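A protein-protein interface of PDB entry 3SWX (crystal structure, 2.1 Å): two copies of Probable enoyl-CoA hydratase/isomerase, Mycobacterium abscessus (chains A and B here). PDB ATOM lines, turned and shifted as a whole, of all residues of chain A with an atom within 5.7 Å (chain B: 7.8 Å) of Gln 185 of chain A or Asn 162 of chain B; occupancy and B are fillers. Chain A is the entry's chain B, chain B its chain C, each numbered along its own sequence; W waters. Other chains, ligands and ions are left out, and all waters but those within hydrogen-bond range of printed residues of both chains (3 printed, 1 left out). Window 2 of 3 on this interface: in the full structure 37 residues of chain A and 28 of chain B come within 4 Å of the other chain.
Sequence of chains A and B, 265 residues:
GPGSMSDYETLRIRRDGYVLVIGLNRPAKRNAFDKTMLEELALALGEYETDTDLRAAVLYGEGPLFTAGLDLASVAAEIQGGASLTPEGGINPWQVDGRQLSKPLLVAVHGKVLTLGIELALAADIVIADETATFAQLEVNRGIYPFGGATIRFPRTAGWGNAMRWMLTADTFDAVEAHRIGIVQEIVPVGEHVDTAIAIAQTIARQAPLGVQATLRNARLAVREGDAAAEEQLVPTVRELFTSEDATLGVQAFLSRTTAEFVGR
O of His 179 of chain A lies within hydrogen-bond range of NH1 of Arg 180 of chain B, at 3.1 Å. NE1 of Trp 160 of chain B sits at hydrogen-bond distance from OD1 of Asp 125 of chain A, at 2.8 Å. The side-chain amide nitrogen (NE2) of Gln 185 of chain A sits at hydrogen-bond distance from the side-chain amide oxygen (OD1) of Asn 162 of chain B.
The side-chain amide oxygen of Asn 162 of chain B lies within hydrogen-bond range of the guanidinium group of Arg 180 of chain B (3.4 Å). ND1 of His 179 of chain A lies within hydrogen-bond range of O of Val 184 of chain A, 3.0 Å away. The side-chain carboxylate (OE1) of Glu 177 of chain B is in salt-bridge range of the guanidinium group (NE) of Arg 180 of chain B, 3.0 Å away. The backbone NH (N) of Gln 185 of chain A lies within hydrogen-bond range of the backbone carbonyl oxygen (O) of Val 127 of chain A (2.8 Å). O of Ala 158 of chain B lies within hydrogen-bond range of ND2 of Asn 162 of chain B (3.1 Å). O of Gly 182 of chain A is in hydrogen-bond range of NE2 of Gln 185 of chain A, 3.0 Å away.
Among the printed residues, pairs that only touch across the chains: Asp 125 of chain A with Gly 161 of chain B, Asp 125 of chain A with Met 164 of chain B, Ile 126 of chain A with Arg 165 of chain B, Gly 182 of chain A with Asn 162 of chain B, Gln 185 of chain A with Gly 161 of chain B and Gln 185 of chain A with Arg 180 of chain B.
Gln 185 of chain A touches just these residues of chain B: Gly 161 (3.4 Å), Asn 162 (3.1 Å) and Arg 180 (3.9 Å). Printed residues of chain A within 4 Å of Gly 161 of chain B: Asp 125 and Gln 185. Of the printed residues of chain B, His 179 of chain A touches Arg 180. Of the printed residues of chain A, Trp 160 of chain B touches Asp 125. Printed residues of chain A within 4 Å of Arg 165 of chain B: Ile 126 (3.8 Å). Printed residues of chain B within 4 Å of Gly 182 of chain A: Asn 162. Val 127 of chain A touches none of the printed residues of chain B. The nearest printed residue of chain A that does not touch Asn 162 of chain B is Val 184 of chain A (4.6 Å).
Hydrophobic or aromatic side chains of chain B that line the printed part of chain A: Trp 160 and Met 164. Of the 11 printed residues of chain A, 5 touch a printed residue of chain B. Hydrophobic or aromatic side chains of chain A that line the printed part of chain B: Ile 126 and His 179. Among the printed residues, 9 pairs touch across the chains. Among the printed residues, no Asp or Glu carboxylate lies within 4 Å of a Lys or Arg side-chain nitrogen of the other chain.
Positions printed for both chains: 182 and 183. Of the 9 pairs that touch across the chains among the printed residues, none has its exchanged pair printed and touching as well.
Water W3 bridges OE1 of Glu 186 of chain A and NH2 of Arg 165 of chain B. Water W1 lies within hydrogen-bond range of O of Gly 182 of chain A (2.7 Å), N of Asn 162 of chain B (3.0 Å), O of Ala 158 of chain B (3.2 Å) and N of Gly 161 of chain B (3.5 Å). Water W2 bridges O of Gln 185 of chain A (2.8 Å) and OE2 of Glu 177 of chain B (3.3 Å).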
ATOM      1  N   ASP A 125      23.401   0.127  19.068  1.00  0.00           N
ATOM      2  CA  ASP A 125      23.140  -0.375  17.727  1.00  0.00           C
ATOM      3  C   ASP A 125      22.557  -1.770  17.724  1.00  0.00           C
ATOM      4  O   ASP A 125      21.821  -2.116  16.815  1.00  0.00           O
ATOM      5  CB  ASP A 125      24.419  -0.311  16.889  1.00  0.00           C
ATOM      6  CG  ASP A 125      24.999   1.062  16.878  1.00  0.00           C
ATOM      7  OD1 ASP A 125      24.263   1.992  16.455  1.00  0.00           O
ATOM      8  OD2 ASP A 125      26.143   1.225  17.356  1.00  0.00           O
ATOM      9  N   ILE A 126      22.870  -2.564  18.741  1.00  0.00           N
ATOM     10  CA  ILE A 126      22.384  -3.954  18.818  1.00  0.00           C
ATOM     11  C   ILE A 126      22.161  -4.296  20.275  1.00  0.00           C
ATOM     12  O   ILE A 126      23.012  -3.995  21.137  1.00  0.00           O
ATOM     13  CB  ILE A 126      23.379  -5.004  18.182  1.00  0.00           C
ATOM     14  CG1 ILE A 126      23.654  -4.725  16.693  1.00  0.00           C
ATOM     15  CG2 ILE A 126      22.814  -6.451  18.298  1.00  0.00           C
ATOM     16  CD1 ILE A 126      24.937  -5.340  16.211  1.00  0.00           C
ATOM     17  N   VAL A 127      21.013  -4.911  20.564  1.00  0.00           N
ATOM     18  CA  VAL A 127      20.630  -5.199  21.942  1.00  0.00           C
ATOM     19  C   VAL A 127      20.364  -6.689  22.055  1.00  0.00           C
ATOM     20  O   VAL A 127      19.579  -7.256  21.274  1.00  0.00           O
ATOM     21  CB  VAL A 127      19.384  -4.388  22.402  1.00  0.00           C
ATOM     22  CG1 VAL A 127      18.955  -4.769  23.841  1.00  0.00           C
ATOM     23  CG2 VAL A 127      19.639  -2.878  22.311  1.00  0.00           C
ATOM     24  N   ILE A 128      21.027  -7.313  23.024  1.00  0.00           N
ATOM     25  CA  ILE A 128      20.844  -8.720  23.311  1.00  0.00           C
ATOM     26  C   ILE A 128      20.313  -8.840  24.726  1.00  0.00           C
ATOM     27  O   ILE A 128      20.889  -8.247  25.655  1.00  0.00           O
ATOM     28  CB  ILE A 128      22.171  -9.490  23.243  1.00  0.00           C
ATOM     29  CG1 ILE A 128      22.875  -9.244  21.906  1.00  0.00           C
ATOM     30  CG2 ILE A 128      21.924 -10.987  23.523  1.00  0.00           C
ATOM     31  CD1 ILE A 128      22.105  -9.745  20.673  1.00  0.00           C
ATOM     32  N   HIS A 179      11.419  -7.927  22.247  1.00  0.00           N
ATOM     33  CA  HIS A 179      11.909  -8.513  21.020  1.00  0.00           C
ATOM     34  C   HIS A 179      10.873  -8.409  19.901  1.00  0.00           C
ATOM     35  O   HIS A 179      11.224  -8.136  18.744  1.00  0.00           O
ATOM     36  CB  HIS A 179      12.263  -9.971  21.298  1.00  0.00           C
ATOM     37  CG  HIS A 179      12.676 -10.742  20.094  1.00  0.00           C
ATOM     38  ND1 HIS A 179      13.821 -10.449  19.387  1.00  0.00           N
ATOM     39  CD2 HIS A 179      12.134 -11.828  19.498  1.00  0.00           C
ATOM     40  CE1 HIS A 179      13.957 -11.314  18.398  1.00  0.00           C
ATOM     41  NE2 HIS A 179      12.950 -12.161  18.444  1.00  0.00           N
ATOM     42  N   GLY A 182      10.907  -4.824  18.569  1.00  0.00           N
ATOM     43  CA  GLY A 182      12.129  -4.387  17.891  1.00  0.00           C
ATOM     44  C   GLY A 182      13.238  -3.779  18.732  1.00  0.00           C
ATOM     45  O   GLY A 182      14.306  -3.454  18.184  1.00  0.00           O
ATOM     46  N   ILE A 183      13.011  -3.599  20.033  1.00  0.00           N
ATOM     47  CA  ILE A 183      14.054  -3.063  20.928  1.00  0.00           C
ATOM     48  C   ILE A 183      15.180  -4.080  21.159  1.00  0.00           C
ATOM     49  O   ILE A 183      16.342  -3.720  21.275  1.00  0.00           O
ATOM     50  CB  ILE A 183      13.528  -2.763  22.365  1.00  0.00           C
ATOM     51  CG1 ILE A 183      12.498  -1.669  22.404  1.00  0.00           C
ATOM     52  CG2 ILE A 183      14.676  -2.307  23.281  1.00  0.00           C
ATOM     53  CD1 ILE A 183      12.008  -1.458  23.906  1.00  0.00           C
ATOM     54  N   VAL A 184      14.812  -5.349  21.279  1.00  0.00           N
ATOM     55  CA  VAL A 184      15.768  -6.418  21.541  1.00  0.00           C
ATOM     56  C   VAL A 184      15.928  -7.262  20.282  1.00  0.00           C
ATOM     57  O   VAL A 184      14.933  -7.728  19.732  1.00  0.00           O
ATOM     58  CB  VAL A 184      15.251  -7.319  22.682  1.00  0.00           C
ATOM     59  CG1 VAL A 184      16.031  -8.665  22.723  1.00  0.00           C
ATOM     60  CG2 VAL A 184      15.351  -6.587  24.005  1.00  0.00           C
ATOM     61  N   GLN A 185      17.162  -7.477  19.839  1.00  0.00           N
ATOM     62  CA  GLN A 185      17.411  -8.192  18.579  1.00  0.00           C
ATOM     63  C   GLN A 185      17.416  -9.694  18.768  1.00  0.00           C
ATOM     64  O   GLN A 185      17.109 -10.441  17.854  1.00  0.00           O
ATOM     65  CB  GLN A 185      18.733  -7.773  17.932  1.00  0.00           C
ATOM     66  CG  GLN A 185      18.640  -6.490  17.128  1.00  0.00           C
ATOM     67  CD  GLN A 185      18.104  -5.334  17.942  1.00  0.00           C
ATOM     68  OE1 GLN A 185      18.821  -4.748  18.766  1.00  0.00           O
ATOM     69  NE2 GLN A 185      16.834  -4.993  17.717  1.00  0.00           N
ATOM     70  N   GLU A 186      17.765 -10.146  19.959  1.00  0.00           N
ATOM     71  CA  GLU A 186      17.851 -11.571  20.195  1.00  0.00           C
ATOM     72  C   GLU A 186      17.744 -11.841  21.686  1.00  0.00           C
ATOM     73  O   GLU A 186      18.281 -11.086  22.512  1.00  0.00           O
ATOM     74  CB  GLU A 186      19.162 -12.122  19.618  1.00  0.00           C
ATOM     75  CG  GLU A 186      19.266 -13.635  19.711  1.00  0.00           C
ATOM     76  CD  GLU A 186      20.580 -14.199  19.174  1.00  0.00           C
ATOM     77  OE1 GLU A 186      21.395 -13.440  18.560  1.00  0.00           O
ATOM     78  OE2 GLU A 186      20.781 -15.426  19.388  1.00  0.00           O
ATOM     79  N   ILE A 187      17.000 -12.901  22.006  1.00  0.00           N
ATOM     80  CA  ILE A 187      16.868 -13.397  23.347  1.00  0.00           C
ATOM     81  C   ILE A 187      17.620 -14.729  23.460  1.00  0.00           C
ATOM     82  O   ILE A 187      17.410 -15.643  22.660  1.00  0.00           O
ATOM     83  CB  ILE A 187      15.406 -13.658  23.719  1.00  0.00           C
ATOM     84  CG1 ILE A 187      14.529 -12.416  23.502  1.00  0.00           C
ATOM     85  CG2 ILE A 187      15.304 -14.139  25.189  1.00  0.00           C
ATOM     86  CD1 ILE A 187      13.048 -12.755  23.545  1.00  0.00           C
ATOM     87  N   PHE B 154      16.632   0.318   5.593  1.00  0.00           N
ATOM     88  CA  PHE B 154      16.644  -0.861   6.450  1.00  0.00           C
ATOM     89  C   PHE B 154      16.309  -0.435   7.890  1.00  0.00           C
ATOM     90  O   PHE B 154      15.430  -1.017   8.484  1.00  0.00           O
ATOM     91  CB  PHE B 154      17.996  -1.574   6.363  1.00  0.00           C
ATOM     92  CG  PHE B 154      17.970  -3.054   6.696  1.00  0.00           C
ATOM     93  CD1 PHE B 154      17.042  -3.609   7.575  1.00  0.00           C
ATOM     94  CD2 PHE B 154      18.962  -3.874   6.172  1.00  0.00           C
ATOM     95  CE1 PHE B 154      17.083  -4.957   7.887  1.00  0.00           C
ATOM     96  CE2 PHE B 154      19.023  -5.226   6.472  1.00  0.00           C
ATOM     97  CZ  PHE B 154      18.087  -5.777   7.325  1.00  0.00           C
ATOM     98  N   PRO B 155      16.951   0.621   8.423  1.00  0.00           N
ATOM     99  CA  PRO B 155      16.531   1.075   9.747  1.00  0.00           C
ATOM    100  C   PRO B 155      15.085   1.545   9.847  1.00  0.00           C
ATOM    101  O   PRO B 155      14.435   1.314  10.873  1.00  0.00           O
ATOM    102  CB  PRO B 155      17.523   2.208  10.051  1.00  0.00           C
ATOM    103  CG  PRO B 155      18.720   1.821   9.317  1.00  0.00           C
ATOM    104  CD  PRO B 155      18.186   1.311   8.011  1.00  0.00           C
ATOM    105  N   THR B 157      12.476   0.467   7.985  1.00  0.00           N
ATOM    106  CA  THR B 157      11.638  -0.739   7.935  1.00  0.00           C
ATOM    107  C   THR B 157      11.739  -1.644   9.176  1.00  0.00           C
ATOM    108  O   THR B 157      10.718  -2.008   9.765  1.00  0.00           O
ATOM    109  CB  THR B 157      11.950  -1.563   6.666  1.00  0.00           C
ATOM    110  OG1 THR B 157      11.596  -0.791   5.508  1.00  0.00           O
ATOM    111  CG2 THR B 157      11.193  -2.878   6.635  1.00  0.00           C
ATOM    112  N   ALA B 158      12.962  -1.987   9.567  1.00  0.00           N
ATOM    113  CA  ALA B 158      13.222  -3.008  10.585  1.00  0.00           C
ATOM    114  C   ALA B 158      13.427  -2.439  11.974  1.00  0.00           C
ATOM    115  O   ALA B 158      13.426  -3.159  12.957  1.00  0.00           O
ATOM    116  CB  ALA B 158      14.472  -3.850  10.161  1.00  0.00           C
ATOM    117  N   GLY B 159      13.627  -1.136  12.057  1.00  0.00           N
ATOM    118  CA  GLY B 159      14.123  -0.532  13.282  1.00  0.00           C
ATOM    119  C   GLY B 159      15.637  -0.496  13.223  1.00  0.00           C
ATOM    120  O   GLY B 159      16.283  -1.324  12.580  1.00  0.00           O
ATOM    121  N   TRP B 160      16.223   0.452  13.932  1.00  0.00           N
ATOM    122  CA  TRP B 160      17.677   0.635  13.895  1.00  0.00           C
ATOM    123  C   TRP B 160      18.445  -0.632  14.299  1.00  0.00           C
ATOM    124  O   TRP B 160      19.304  -1.085  13.564  1.00  0.00           O
ATOM    125  CB  TRP B 160      18.054   1.811  14.796  1.00  0.00           C
ATOM    126  CG  TRP B 160      19.487   2.167  14.810  1.00  0.00           C
ATOM    127  CD1 TRP B 160      20.444   1.642  15.618  1.00  0.00           C
ATOM    128  CD2 TRP B 160      20.139   3.145  13.998  1.00  0.00           C
ATOM    129  NE1 TRP B 160      21.663   2.230  15.367  1.00  0.00           N
ATOM    130  CE2 TRP B 160      21.504   3.156  14.371  1.00  0.00           C
ATOM    131  CE3 TRP B 160      19.714   3.997  12.977  1.00  0.00           C
ATOM    132  CZ2 TRP B 160      22.443   3.992  13.764  1.00  0.00           C
ATOM    133  CZ3 TRP B 160      20.653   4.836  12.376  1.00  0.00           C
ATOM    134  CH2 TRP B 160      22.002   4.830  12.778  1.00  0.00           C
ATOM    135  N   GLY B 161      18.126  -1.185  15.468  1.00  0.00           N
ATOM    136  CA  GLY B 161      18.821  -2.356  16.010  1.00  0.00           C
ATOM    137  C   GLY B 161      18.754  -3.584  15.118  1.00  0.00           C
ATOM    138  O   GLY B 161      19.768  -4.198  14.834  1.00  0.00           O
ATOM    139  N   ASN B 162      17.561  -3.914  14.644  1.00  0.00           N
ATOM    140  CA  ASN B 162      17.394  -5.029  13.712  1.00  0.00           C
ATOM    141  C   ASN B 162      18.167  -4.815  12.412  1.00  0.00           C
ATOM    142  O   ASN B 162      18.825  -5.740  11.936  1.00  0.00           O
ATOM    143  CB  ASN B 162      15.919  -5.269  13.401  1.00  0.00           C
ATOM    144  CG  ASN B 162      15.171  -5.954  14.532  1.00  0.00           C
ATOM    145  OD1 ASN B 162      15.757  -6.652  15.348  1.00  0.00           O
ATOM    146  ND2 ASN B 162      13.839  -5.776  14.556  1.00  0.00           N
ATOM    147  N   ALA B 163      18.109  -3.606  11.850  1.00  0.00           N
ATOM    148  CA  ALA B 163      18.926  -3.279  10.679  1.00  0.00           C
ATOM    149  C   ALA B 163      20.439  -3.374  10.923  1.00  0.00           C
ATOM    150  O   ALA B 163      21.161  -3.952  10.126  1.00  0.00           O
ATOM    151  CB  ALA B 163      18.573  -1.899  10.113  1.00  0.00           C
ATOM    152  N   MET B 164      20.919  -2.818  12.016  1.00  0.00           N
ATOM    153  CA  MET B 164      22.354  -2.840  12.274  1.00  0.00           C
ATOM    154  C   MET B 164      22.904  -4.244  12.591  1.00  0.00           C
ATOM    155  O   MET B 164      24.052  -4.541  12.254  1.00  0.00           O
ATOM    156  CB  MET B 164      22.698  -1.843  13.375  1.00  0.00           C
ATOM    157  CG  MET B 164      22.455  -0.399  12.962  1.00  0.00           C
ATOM    158  SD  MET B 164      23.529   0.067  11.572  1.00  0.00           S
ATOM    159  CE  MET B 164      22.745   1.587  11.006  1.00  0.00           C
ATOM    160  N   ARG B 165      22.091  -5.114  13.202  1.00  0.00           N
ATOM    161  CA  ARG B 165      22.502  -6.504  13.440  1.00  0.00           C
ATOM    162  C   ARG B 165      22.982  -7.187  12.165  1.00  0.00           C
ATOM    163  O   ARG B 165      23.930  -7.966  12.198  1.00  0.00           O
ATOM    164  CB  ARG B 165      21.346  -7.284  14.072  1.00  0.00           C
ATOM    165  CG  ARG B 165      21.550  -8.788  14.232  1.00  0.00           C
ATOM    166  CD  ARG B 165      22.669  -9.084  15.162  1.00  0.00           C
ATOM    167  NE  ARG B 165      22.900 -10.532  15.252  1.00  0.00           N
ATOM    168  CZ  ARG B 165      23.623 -11.252  14.408  1.00  0.00           C
ATOM    169  NH1 ARG B 165      24.208 -10.705  13.342  1.00  0.00           N
ATOM    170  NH2 ARG B 165      23.747 -12.541  14.631  1.00  0.00           N
ATOM    171  N   TRP B 166      22.348  -6.879  11.033  1.00  0.00           N
ATOM    172  CA  TRP B 166      22.700  -7.497   9.757  1.00  0.00           C
ATOM    173  C   TRP B 166      23.658  -6.633   8.932  1.00  0.00           C
ATOM    174  O   TRP B 166      24.616  -7.155   8.320  1.00  0.00           O
ATOM    175  CB  TRP B 166      21.417  -7.850   8.992  1.00  0.00           C
ATOM    176  CG  TRP B 166      20.495  -8.663   9.863  1.00  0.00           C
ATOM    177  CD1 TRP B 166      19.246  -8.310  10.321  1.00  0.00           C
ATOM    178  CD2 TRP B 166      20.796  -9.928  10.469  1.00  0.00           C
ATOM    179  NE1 TRP B 166      18.744  -9.306  11.137  1.00  0.00           N
ATOM    180  CE2 TRP B 166      19.687 -10.293  11.263  1.00  0.00           C
ATOM    181  CE3 TRP B 166      21.894 -10.795  10.410  1.00  0.00           C
ATOM    182  CZ2 TRP B 166      19.643 -11.494  11.973  1.00  0.00           C
ATOM    183  CZ3 TRP B 166      21.847 -11.986  11.130  1.00  0.00           C
ATOM    184  CH2 TRP B 166      20.726 -12.324  11.888  1.00  0.00           C
ATOM    185  N   MET B 167      23.454  -5.320   8.939  1.00  0.00           N
ATOM    186  CA  MET B 167      24.325  -4.444   8.148  1.00  0.00           C
ATOM    187  C   MET B 167      25.746  -4.328   8.691  1.00  0.00           C
ATOM    188  O   MET B 167      26.677  -4.165   7.931  1.00  0.00           O
ATOM    189  CB  MET B 167      23.718  -3.042   7.981  1.00  0.00           C
ATOM    190  CG  MET B 167      22.386  -2.990   7.200  1.00  0.00           C
ATOM    191  SD  MET B 167      21.952  -1.277   6.725  1.00  0.00           S
ATOM    192  CE  MET B 167      21.948  -0.391   8.288  1.00  0.00           C
ATOM    193  N   LEU B 168      25.928  -4.392  10.002  1.00  0.00           N
ATOM    194  CA  LEU B 168      27.263  -4.159  10.554  1.00  0.00           C
ATOM    195  C   LEU B 168      28.095  -5.450  10.582  1.00  0.00           C
ATOM    196  O   LEU B 168      29.334  -5.404  10.685  1.00  0.00           O
ATOM    197  CB  LEU B 168      27.172  -3.552  11.970  1.00  0.00           C
ATOM    198  CG  LEU B 168      26.528  -2.168  12.129  1.00  0.00           C
ATOM    199  CD1 LEU B 168      26.527  -1.732  13.610  1.00  0.00           C
ATOM    200  CD2 LEU B 168      27.234  -1.111  11.243  1.00  0.00           C
ATOM    201  N   PHE B 173      20.938 -14.017   7.079  1.00  0.00           N
ATOM    202  CA  PHE B 173      19.681 -14.212   7.770  1.00  0.00           C
ATOM    203  C   PHE B 173      18.647 -14.818   6.813  1.00  0.00           C
ATOM    204  O   PHE B 173      18.769 -14.679   5.606  1.00  0.00           O
ATOM    205  CB  PHE B 173      19.209 -12.920   8.468  1.00  0.00           C
ATOM    206  CG  PHE B 173      19.031 -11.737   7.572  1.00  0.00           C
ATOM    207  CD1 PHE B 173      20.114 -10.939   7.228  1.00  0.00           C
ATOM    208  CD2 PHE B 173      17.744 -11.360   7.130  1.00  0.00           C
ATOM    209  CE1 PHE B 173      19.952  -9.828   6.422  1.00  0.00           C
ATOM    210  CE2 PHE B 173      17.570 -10.235   6.323  1.00  0.00           C
ATOM    211  CZ  PHE B 173      18.682  -9.470   5.972  1.00  0.00           C
ATOM    212  N   GLU B 177      13.466 -14.542   9.562  1.00  0.00           N
ATOM    213  CA  GLU B 177      13.974 -13.269  10.137  1.00  0.00           C
ATOM    214  C   GLU B 177      13.577 -12.061   9.266  1.00  0.00           C
ATOM    215  O   GLU B 177      13.061 -11.059   9.777  1.00  0.00           O
ATOM    216  CB  GLU B 177      15.499 -13.353  10.321  1.00  0.00           C
ATOM    217  CG  GLU B 177      16.185 -12.154  10.973  1.00  0.00           C
ATOM    218  CD  GLU B 177      15.747 -11.850  12.406  1.00  0.00           C
ATOM    219  OE1 GLU B 177      14.945 -12.575  12.992  1.00  0.00           O
ATOM    220  OE2 GLU B 177      16.202 -10.820  12.951  1.00  0.00           O
ATOM    221  N   ARG B 180      10.011 -11.312   9.932  1.00  0.00           N
ATOM    222  CA  ARG B 180       9.878 -10.808  11.303  1.00  0.00           C
ATOM    223  C   ARG B 180      10.192  -9.322  11.374  1.00  0.00           C
ATOM    224  O   ARG B 180       9.473  -8.560  12.002  1.00  0.00           O
ATOM    225  CB  ARG B 180      10.814 -11.564  12.248  1.00  0.00           C
ATOM    226  CG  ARG B 180      10.413 -11.452  13.731  1.00  0.00           C
ATOM    227  CD  ARG B 180      11.470 -12.085  14.663  1.00  0.00           C
ATOM    228  NE  ARG B 180      12.738 -11.364  14.635  1.00  0.00           N
ATOM    229  CZ  ARG B 180      13.026 -10.284  15.369  1.00  0.00           C
ATOM    230  NH1 ARG B 180      12.132  -9.764  16.207  1.00  0.00           N
ATOM    231  NH2 ARG B 180      14.215  -9.718  15.266  1.00  0.00           N
ATOM    232  N   ILE B 181      11.251  -8.913  10.688  1.00  0.00           N
ATOM    233  CA  ILE B 181      11.728  -7.554  10.790  1.00  0.00           C
ATOM    234  C   ILE B 181      11.148  -6.619   9.725  1.00  0.00           C
ATOM    235  O   ILE B 181      11.475  -5.440   9.722  1.00  0.00           O
ATOM    236  CB  ILE B 181      13.284  -7.492  10.887  1.00  0.00           C
ATOM    237  CG1 ILE B 181      13.967  -7.760   9.548  1.00  0.00           C
ATOM    238  CG2 ILE B 181      13.796  -8.484  11.960  1.00  0.00           C
ATOM    239  CD1 ILE B 181      15.452  -7.973   9.680  1.00  0.00           C
ATOM    240  N   GLY B 182      10.269  -7.115   8.851  1.00  0.00           N
ATOM    241  CA  GLY B 182       9.446  -6.223   8.013  1.00  0.00           C
ATOM    242  C   GLY B 182       9.862  -6.056   6.564  1.00  0.00           C
ATOM    243  O   GLY B 182       9.146  -5.414   5.801  1.00  0.00           O
ATOM    244  N   ILE B 183      11.005  -6.646   6.175  1.00  0.00           N
ATOM    245  CA  ILE B 183      11.499  -6.588   4.803  1.00  0.00           C
ATOM    246  C   ILE B 183      10.644  -7.424   3.847  1.00  0.00           C
ATOM    247  O   ILE B 183      10.340  -7.008   2.733  1.00  0.00           O
ATOM    248  CB  ILE B 183      12.909  -7.173   4.684  1.00  0.00           C
ATOM    249  CG1 ILE B 183      13.930  -6.352   5.448  1.00  0.00           C
ATOM    250  CG2 ILE B 183      13.360  -7.214   3.218  1.00  0.00           C
ATOM    251  CD1 ILE B 183      15.365  -7.031   5.320  1.00  0.00           C
HETATM  252  O   HOH W   1      14.995  -2.695  15.674  1.00  0.00           O
HETATM  253  O   HOH W   2      18.356 -10.463  15.360  1.00  0.00           O
HETATM  254  O   HOH W   3      23.508 -14.219  17.515  1.00  0.00           O
